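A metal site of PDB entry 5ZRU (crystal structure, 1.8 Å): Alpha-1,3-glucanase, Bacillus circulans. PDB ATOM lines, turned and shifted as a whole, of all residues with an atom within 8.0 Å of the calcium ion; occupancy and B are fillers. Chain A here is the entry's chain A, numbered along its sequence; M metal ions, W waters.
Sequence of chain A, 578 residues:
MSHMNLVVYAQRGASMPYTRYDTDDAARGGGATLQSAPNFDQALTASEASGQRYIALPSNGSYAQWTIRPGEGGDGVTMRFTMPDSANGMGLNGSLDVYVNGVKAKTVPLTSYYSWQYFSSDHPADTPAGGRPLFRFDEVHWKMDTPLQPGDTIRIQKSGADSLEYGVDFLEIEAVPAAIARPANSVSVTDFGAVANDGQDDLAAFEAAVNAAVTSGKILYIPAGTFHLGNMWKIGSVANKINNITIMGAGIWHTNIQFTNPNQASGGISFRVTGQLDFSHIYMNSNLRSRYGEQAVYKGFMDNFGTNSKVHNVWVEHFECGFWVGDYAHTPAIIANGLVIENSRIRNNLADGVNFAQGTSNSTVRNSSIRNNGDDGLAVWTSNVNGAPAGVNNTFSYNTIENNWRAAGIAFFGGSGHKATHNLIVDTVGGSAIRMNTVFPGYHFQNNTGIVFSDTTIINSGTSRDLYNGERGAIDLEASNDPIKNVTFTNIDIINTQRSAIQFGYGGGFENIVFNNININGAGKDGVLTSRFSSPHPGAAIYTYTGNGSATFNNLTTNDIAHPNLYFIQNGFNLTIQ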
ATOM      1  N   ARG A  20     -14.089  10.772 -11.278  1.00  0.00           N
ATOM      2  CA  ARG A  20     -15.104  11.805 -11.394  1.00  0.00           C
ATOM      3  C   ARG A  20     -15.595  12.271 -10.038  1.00  0.00           C
ATOM      4  O   ARG A  20     -15.862  11.469  -9.147  1.00  0.00           O
ATOM      5  CB  ARG A  20     -16.303  11.334 -12.212  1.00  0.00           C
ATOM      6  CG  ARG A  20     -17.317  12.462 -12.263  1.00  0.00           C
ATOM      7  CD  ARG A  20     -18.372  12.254 -13.239  1.00  0.00           C
ATOM      8  NE  ARG A  20     -17.833  12.037 -14.568  1.00  0.00           N
ATOM      9  CZ  ARG A  20     -18.623  11.787 -15.601  1.00  0.00           C
ATOM     10  NH1 ARG A  20     -19.932  11.760 -15.410  1.00  0.00           N
ATOM     11  NH2 ARG A  20     -18.104  11.578 -16.805  1.00  0.00           N
ATOM     12  N   TYR A  21     -15.716  13.585  -9.903  1.00  0.00           N
ATOM     13  CA  TYR A  21     -16.371  14.246  -8.785  1.00  0.00           C
ATOM     14  C   TYR A  21     -17.643  14.869  -9.331  1.00  0.00           C
ATOM     15  O   TYR A  21     -17.595  15.949  -9.944  1.00  0.00           O
ATOM     16  CB  TYR A  21     -15.411  15.270  -8.161  1.00  0.00           C
ATOM     17  CG  TYR A  21     -14.302  14.553  -7.433  1.00  0.00           C
ATOM     18  CD1 TYR A  21     -13.187  14.068  -8.110  1.00  0.00           C
ATOM     19  CD2 TYR A  21     -14.400  14.305  -6.071  1.00  0.00           C
ATOM     20  CE1 TYR A  21     -12.204  13.370  -7.439  1.00  0.00           C
ATOM     21  CE2 TYR A  21     -13.422  13.630  -5.395  1.00  0.00           C
ATOM     22  CZ  TYR A  21     -12.322  13.168  -6.076  1.00  0.00           C
ATOM     23  OH  TYR A  21     -11.365  12.484  -5.374  1.00  0.00           O
ATOM     24  N   ASP A  22     -18.783  14.193  -9.151  1.00  0.00           N
ATOM     25  CA  ASP A  22     -20.001  14.562  -9.853  1.00  0.00           C
ATOM     26  C   ASP A  22     -20.924  15.372  -8.944  1.00  0.00           C
ATOM     27  O   ASP A  22     -20.601  15.686  -7.795  1.00  0.00           O
ATOM     28  CB  ASP A  22     -20.728  13.325 -10.412  1.00  0.00           C
ATOM     29  CG  ASP A  22     -21.450  13.604 -11.762  1.00  0.00           C
ATOM     30  OD1 ASP A  22     -22.082  14.684 -11.914  1.00  0.00           O
ATOM     31  OD2 ASP A  22     -21.396  12.740 -12.674  1.00  0.00           O
ATOM     32  N   THR A  23     -22.114  15.652  -9.478  1.00  0.00           N
ATOM     33  CA  THR A  23     -22.989  16.661  -8.889  1.00  0.00           C
ATOM     34  C   THR A  23     -23.333  16.351  -7.446  1.00  0.00           C
ATOM     35  O   THR A  23     -23.250  17.214  -6.570  1.00  0.00           O
ATOM     36  CB  THR A  23     -24.257  16.787  -9.741  1.00  0.00           C
ATOM     37  OG1 THR A  23     -23.895  17.160 -11.070  1.00  0.00           O
ATOM     38  CG2 THR A  23     -25.179  17.832  -9.162  1.00  0.00           C
ATOM     39  N   ASP A  24     -23.715  15.102  -7.162  1.00  0.00           N
ATOM     40  CA  ASP A  24     -24.172  14.761  -5.828  1.00  0.00           C
ATOM     41  C   ASP A  24     -23.037  14.592  -4.823  1.00  0.00           C
ATOM     42  O   ASP A  24     -23.311  14.578  -3.617  1.00  0.00           O
ATOM     43  CB  ASP A  24     -25.034  13.494  -5.883  1.00  0.00           C
ATOM     44  CG  ASP A  24     -26.310  13.698  -6.691  1.00  0.00           C
ATOM     45  OD1 ASP A  24     -27.036  14.683  -6.422  1.00  0.00           O
ATOM     46  OD2 ASP A  24     -26.591  12.881  -7.594  1.00  0.00           O
ATOM     47  N   LEU A  34     -29.351  23.030  -6.779  1.00  0.00           N
ATOM     48  CA  LEU A  34     -29.387  21.811  -7.575  1.00  0.00           C
ATOM     49  C   LEU A  34     -30.439  21.961  -8.660  1.00  0.00           C
ATOM     50  O   LEU A  34     -31.602  22.241  -8.372  1.00  0.00           O
ATOM     51  CB  LEU A  34     -29.688  20.606  -6.672  1.00  0.00           C
ATOM     52  CG  LEU A  34     -29.578  19.151  -7.151  1.00  0.00           C
ATOM     53  CD1 LEU A  34     -30.624  18.760  -8.194  1.00  0.00           C
ATOM     54  CD2 LEU A  34     -28.183  18.868  -7.661  1.00  0.00           C
ATOM     55  N   GLN A  35     -30.043  21.800  -9.914  1.00  0.00           N
ATOM     56  CA  GLN A  35     -30.961  21.867 -11.052  1.00  0.00           C
ATOM     57  C   GLN A  35     -31.096  20.468 -11.623  1.00  0.00           C
ATOM     58  O   GLN A  35     -30.083  19.804 -11.846  1.00  0.00           O
ATOM     59  CB  GLN A  35     -30.446  22.817 -12.128  1.00  0.00           C
ATOM     60  CG  GLN A  35     -30.169  24.217 -11.642  1.00  0.00           C
ATOM     61  CD  GLN A  35     -31.422  24.936 -11.224  1.00  0.00           C
ATOM     62  OE1 GLN A  35     -31.507  25.471 -10.123  1.00  0.00           O
ATOM     63  NE2 GLN A  35     -32.412  24.940 -12.103  1.00  0.00           N
ATOM     64  N   ALA A  46     -30.770  21.216 -17.571  1.00  0.00           N
ATOM     65  CA  ALA A  46     -30.332  20.038 -16.841  1.00  0.00           C
ATOM     66  C   ALA A  46     -30.534  18.739 -17.622  1.00  0.00           C
ATOM     67  O   ALA A  46     -29.935  17.726 -17.250  1.00  0.00           O
ATOM     68  CB  ALA A  46     -31.064  19.962 -15.495  1.00  0.00           C
ATOM     69  N   GLU A  48     -29.213  18.012 -20.274  1.00  0.00           N
ATOM     70  CA  GLU A  48     -27.906  17.689 -20.831  1.00  0.00           C
ATOM     71  C   GLU A  48     -26.811  17.552 -19.776  1.00  0.00           C
ATOM     72  O   GLU A  48     -25.646  17.338 -20.147  1.00  0.00           O
ATOM     73  CB  GLU A  48     -27.494  18.749 -21.859  1.00  0.00           C
ATOM     74  CG  GLU A  48     -28.336  18.760 -23.124  1.00  0.00           C
ATOM     75  CD  GLU A  48     -27.735  19.668 -24.170  1.00  0.00           C
ATOM     76  OE1 GLU A  48     -26.830  19.221 -24.925  1.00  0.00           O
ATOM     77  OE2 GLU A  48     -28.136  20.837 -24.227  1.00  0.00           O
ATOM     78  N   ALA A  49     -27.134  17.655 -18.499  1.00  0.00           N
ATOM     79  CA  ALA A  49     -26.158  17.371 -17.454  1.00  0.00           C
ATOM     80  C   ALA A  49     -26.061  15.866 -17.208  1.00  0.00           C
ATOM     81  O   ALA A  49     -27.046  15.128 -17.387  1.00  0.00           O
ATOM     82  CB  ALA A  49     -26.526  18.079 -16.151  1.00  0.00           C
ATOM     83  N   SER A  50     -24.885  15.407 -16.780  1.00  0.00           N
ATOM     84  CA  SER A  50     -24.778  13.994 -16.423  1.00  0.00           C
ATOM     85  C   SER A  50     -25.778  13.690 -15.306  1.00  0.00           C
ATOM     86  O   SER A  50     -25.955  14.479 -14.365  1.00  0.00           O
ATOM     87  CB  SER A  50     -23.349  13.625 -15.983  1.00  0.00           C
ATOM     88  OG  SER A  50     -23.014  14.271 -14.774  1.00  0.00           O
ATOM     89  N   GLY A  51     -26.479  12.574 -15.438  1.00  0.00           N
ATOM     90  CA  GLY A  51     -27.513  12.221 -14.481  1.00  0.00           C
ATOM     91  C   GLY A  51     -28.661  13.205 -14.421  1.00  0.00           C
ATOM     92  O   GLY A  51     -29.456  13.166 -13.482  1.00  0.00           O
ATOM     93  N   GLN A  52     -28.757  14.082 -15.438  1.00  0.00           N
ATOM     94  CA  GLN A  52     -29.806  15.105 -15.523  1.00  0.00           C
ATOM     95  C   GLN A  52     -29.838  15.988 -14.278  1.00  0.00           C
ATOM     96  O   GLN A  52     -30.906  16.423 -13.827  1.00  0.00           O
ATOM     97  CB  GLN A  52     -31.167  14.480 -15.811  1.00  0.00           C
ATOM     98  CG  GLN A  52     -31.199  13.666 -17.113  1.00  0.00           C
ATOM     99  CD  GLN A  52     -30.571  12.285 -16.964  1.00  0.00           C
ATOM    100  OE1 GLN A  52     -30.878  11.552 -16.012  1.00  0.00           O
ATOM    101  NE2 GLN A  52     -29.695  11.928 -17.887  1.00  0.00           N
ATOM    102  N   ARG A  53     -28.665  16.271 -13.718  1.00  0.00           N
ATOM    103  CA  ARG A  53     -28.533  17.076 -12.508  1.00  0.00           C
ATOM    104  C   ARG A  53     -27.225  17.863 -12.582  1.00  0.00           C
ATOM    105  O   ARG A  53     -26.205  17.306 -12.961  1.00  0.00           O
ATOM    106  CB  ARG A  53     -28.512  16.198 -11.252  1.00  0.00           C
ATOM    107  CG  ARG A  53     -29.810  15.470 -10.964  1.00  0.00           C
ATOM    108  CD  ARG A  53     -29.574  14.261 -10.084  1.00  0.00           C
ATOM    109  NE  ARG A  53     -29.233  14.656  -8.722  1.00  0.00           N
ATOM    110  CZ  ARG A  53     -30.125  15.003  -7.800  1.00  0.00           C
ATOM    111  NH1 ARG A  53     -31.422  15.027  -8.120  1.00  0.00           N
ATOM    112  NH2 ARG A  53     -29.738  15.335  -6.585  1.00  0.00           N
ATOM    113  N   TYR A  54     -27.268  19.147 -12.218  1.00  0.00           N
ATOM    114  CA  TYR A  54     -26.041  19.912 -12.102  1.00  0.00           C
ATOM    115  C   TYR A  54     -26.229  20.987 -11.038  1.00  0.00           C
ATOM    116  O   TYR A  54     -27.338  21.207 -10.544  1.00  0.00           O
ATOM    117  CB  TYR A  54     -25.609  20.526 -13.443  1.00  0.00           C
ATOM    118  CG  TYR A  54     -26.463  21.687 -13.929  1.00  0.00           C
ATOM    119  CD1 TYR A  54     -27.679  21.468 -14.594  1.00  0.00           C
ATOM    120  CD2 TYR A  54     -26.036  23.006 -13.752  1.00  0.00           C
ATOM    121  CE1 TYR A  54     -28.445  22.534 -15.074  1.00  0.00           C
ATOM    122  CE2 TYR A  54     -26.799  24.084 -14.226  1.00  0.00           C
ATOM    123  CZ  TYR A  54     -28.000  23.842 -14.886  1.00  0.00           C
ATOM    124  OH  TYR A  54     -28.753  24.902 -15.350  1.00  0.00           O
ATOM    125  N   ILE A  55     -25.129  21.649 -10.685  1.00  0.00           N
ATOM    126  CA  ILE A  55     -25.156  22.709  -9.673  1.00  0.00           C
ATOM    127  C   ILE A  55     -25.133  24.044 -10.392  1.00  0.00           C
ATOM    128  O   ILE A  55     -24.192  24.355 -11.132  1.00  0.00           O
ATOM    129  CB  ILE A  55     -23.969  22.593  -8.699  1.00  0.00           C
ATOM    130  CG1 ILE A  55     -23.991  21.240  -7.993  1.00  0.00           C
ATOM    131  CG2 ILE A  55     -24.009  23.724  -7.672  1.00  0.00           C
ATOM    132  CD1 ILE A  55     -22.643  20.577  -7.977  1.00  0.00           C
ATOM    133  N   ARG A  80     -16.800  20.050 -16.567  1.00  0.00           N
ATOM    134  CA  ARG A  80     -17.934  20.167 -17.483  1.00  0.00           C
ATOM    135  C   ARG A  80     -18.894  21.196 -16.902  1.00  0.00           C
ATOM    136  O   ARG A  80     -19.337  21.065 -15.744  1.00  0.00           O
ATOM    137  CB  ARG A  80     -18.630  18.826 -17.709  1.00  0.00           C
ATOM    138  CG  ARG A  80     -19.700  18.878 -18.804  1.00  0.00           C
ATOM    139  CD  ARG A  80     -20.132  17.477 -19.200  1.00  0.00           C
ATOM    140  NE  ARG A  80     -20.997  17.488 -20.368  1.00  0.00           N
ATOM    141  CZ  ARG A  80     -22.324  17.442 -20.322  1.00  0.00           C
ATOM    142  NH1 ARG A  80     -22.957  17.376 -19.155  1.00  0.00           N
ATOM    143  NH2 ARG A  80     -23.022  17.450 -21.450  1.00  0.00           N
ATOM    144  N   PHE A 137     -23.742  22.309 -22.650  1.00  0.00           N
ATOM    145  CA  PHE A 137     -22.580  22.106 -21.803  1.00  0.00           C
ATOM    146  C   PHE A 137     -21.304  22.040 -22.639  1.00  0.00           C
ATOM    147  O   PHE A 137     -21.325  21.753 -23.836  1.00  0.00           O
ATOM    148  CB  PHE A 137     -22.743  20.830 -20.945  1.00  0.00           C
ATOM    149  CG  PHE A 137     -23.680  21.001 -19.776  1.00  0.00           C
ATOM    150  CD1 PHE A 137     -25.059  20.887 -19.934  1.00  0.00           C
ATOM    151  CD2 PHE A 137     -23.174  21.292 -18.503  1.00  0.00           C
ATOM    152  CE1 PHE A 137     -25.924  21.056 -18.854  1.00  0.00           C
ATOM    153  CE2 PHE A 137     -24.033  21.468 -17.408  1.00  0.00           C
ATOM    154  CZ  PHE A 137     -25.411  21.353 -17.580  1.00  0.00           C
ATOM    155  N   VAL A 168     -22.167  24.016 -13.017  1.00  0.00           N
ATOM    156  CA  VAL A 168     -21.084  23.036 -12.951  1.00  0.00           C
ATOM    157  C   VAL A 168     -21.688  21.660 -12.829  1.00  0.00           C
ATOM    158  O   VAL A 168     -22.434  21.365 -11.880  1.00  0.00           O
ATOM    159  CB  VAL A 168     -20.125  23.317 -11.778  1.00  0.00           C
ATOM    160  CG1 VAL A 168     -18.987  22.302 -11.780  1.00  0.00           C
ATOM    161  CG2 VAL A 168     -19.568  24.725 -11.887  1.00  0.00           C
ATOM    162  N   ASP A 169     -21.339  20.776 -13.780  1.00  0.00           N
ATOM    163  CA  ASP A 169     -21.802  19.388 -13.766  1.00  0.00           C
ATOM    164  C   ASP A 169     -20.866  18.516 -12.933  1.00  0.00           C
ATOM    165  O   ASP A 169     -21.279  17.929 -11.921  1.00  0.00           O
ATOM    166  CB  ASP A 169     -21.883  18.891 -15.224  1.00  0.00           C
ATOM    167  CG  ASP A 169     -22.600  17.567 -15.368  1.00  0.00           C
ATOM    168  OD1 ASP A 169     -23.062  17.000 -14.350  1.00  0.00           O
ATOM    169  OD2 ASP A 169     -22.687  17.082 -16.527  1.00  0.00           O
ATOM    170  N   PHE A 170     -19.589  18.441 -13.310  1.00  0.00           N
ATOM    171  CA  PHE A 170     -18.653  17.603 -12.580  1.00  0.00           C
ATOM    172  C   PHE A 170     -17.242  18.099 -12.813  1.00  0.00           C
ATOM    173  O   PHE A 170     -16.975  18.900 -13.704  1.00  0.00           O
ATOM    174  CB  PHE A 170     -18.775  16.116 -12.964  1.00  0.00           C
ATOM    175  CG  PHE A 170     -18.569  15.844 -14.442  1.00  0.00           C
ATOM    176  CD1 PHE A 170     -17.297  15.864 -15.005  1.00  0.00           C
ATOM    177  CD2 PHE A 170     -19.644  15.514 -15.257  1.00  0.00           C
ATOM    178  CE1 PHE A 170     -17.096  15.598 -16.376  1.00  0.00           C
ATOM    179  CE2 PHE A 170     -19.449  15.238 -16.621  1.00  0.00           C
ATOM    180  CZ  PHE A 170     -18.181  15.280 -17.179  1.00  0.00           C
ATOM    181  N   ASN A 403     -23.211  11.713 -22.919  1.00  0.00           N
ATOM    182  CA  ASN A 403     -23.777  13.051 -23.156  1.00  0.00           C
ATOM    183  C   ASN A 403     -23.927  13.401 -24.628  1.00  0.00           C
ATOM    184  O   ASN A 403     -23.931  14.572 -24.997  1.00  0.00           O
ATOM    185  CB  ASN A 403     -22.965  14.138 -22.452  1.00  0.00           C
ATOM    186  CG  ASN A 403     -22.859  13.924 -20.959  1.00  0.00           C
ATOM    187  OD1 ASN A 403     -21.771  13.671 -20.436  1.00  0.00           O
ATOM    188  ND2 ASN A 403     -23.981  14.017 -20.258  1.00  0.00           N
ATOM    189  N   ASP A 427     -26.479   8.637 -20.841  1.00  0.00           N
ATOM    190  CA  ASP A 427     -27.045   9.993 -20.865  1.00  0.00           C
ATOM    191  C   ASP A 427     -27.140  10.594 -22.273  1.00  0.00           C
ATOM    192  O   ASP A 427     -26.776  11.748 -22.489  1.00  0.00           O
ATOM    193  CB  ASP A 427     -26.237  10.924 -19.951  1.00  0.00           C
ATOM    194  CG  ASP A 427     -26.433  10.622 -18.478  1.00  0.00           C
ATOM    195  OD1 ASP A 427     -27.483  10.038 -18.139  1.00  0.00           O
ATOM    196  OD2 ASP A 427     -25.542  10.976 -17.672  1.00  0.00           O
HETATM  197 CA    CA M   1     -24.501  15.737 -12.983  1.00  0.00          CA
HETATM  198  O   HOH W   1     -25.063  13.846 -11.489  1.00  0.00           O
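The side-chain carboxylate of Asp 24 lies within salt-bridge range of the guanidinium group of Arg 53 (2.8 Å). The side-chain carboxylate (OD2) of Asp 169 is in salt-bridge range of the guanidinium group (NH1) of Arg 80 (2.7 Å). The guanidinium group of Arg 20 is in salt-bridge range of the side-chain carboxylate of Asp 22.
Five residues have an atom within 4 Å of the calcium ion: Asp 22, Thr 23, Ser 50, Arg 53 and Asp 169. The nearest printed residue that does not touch the calcium ion is Ala 49 (4.4 Å).
The calcium ion is bound by O of Arg 53 (2.3 Å), OD1 of Asp 169 (2.4 Å), O of Ser 50 (2.4 Å), OG1 of Thr 23 (2.5 Å), water W1 (2.5 Å), OG of Ser 50 (2.8 Å) and OD1 of Asp 22 (2.8 Å). The calcium ion has seven donor atoms within binding distance.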
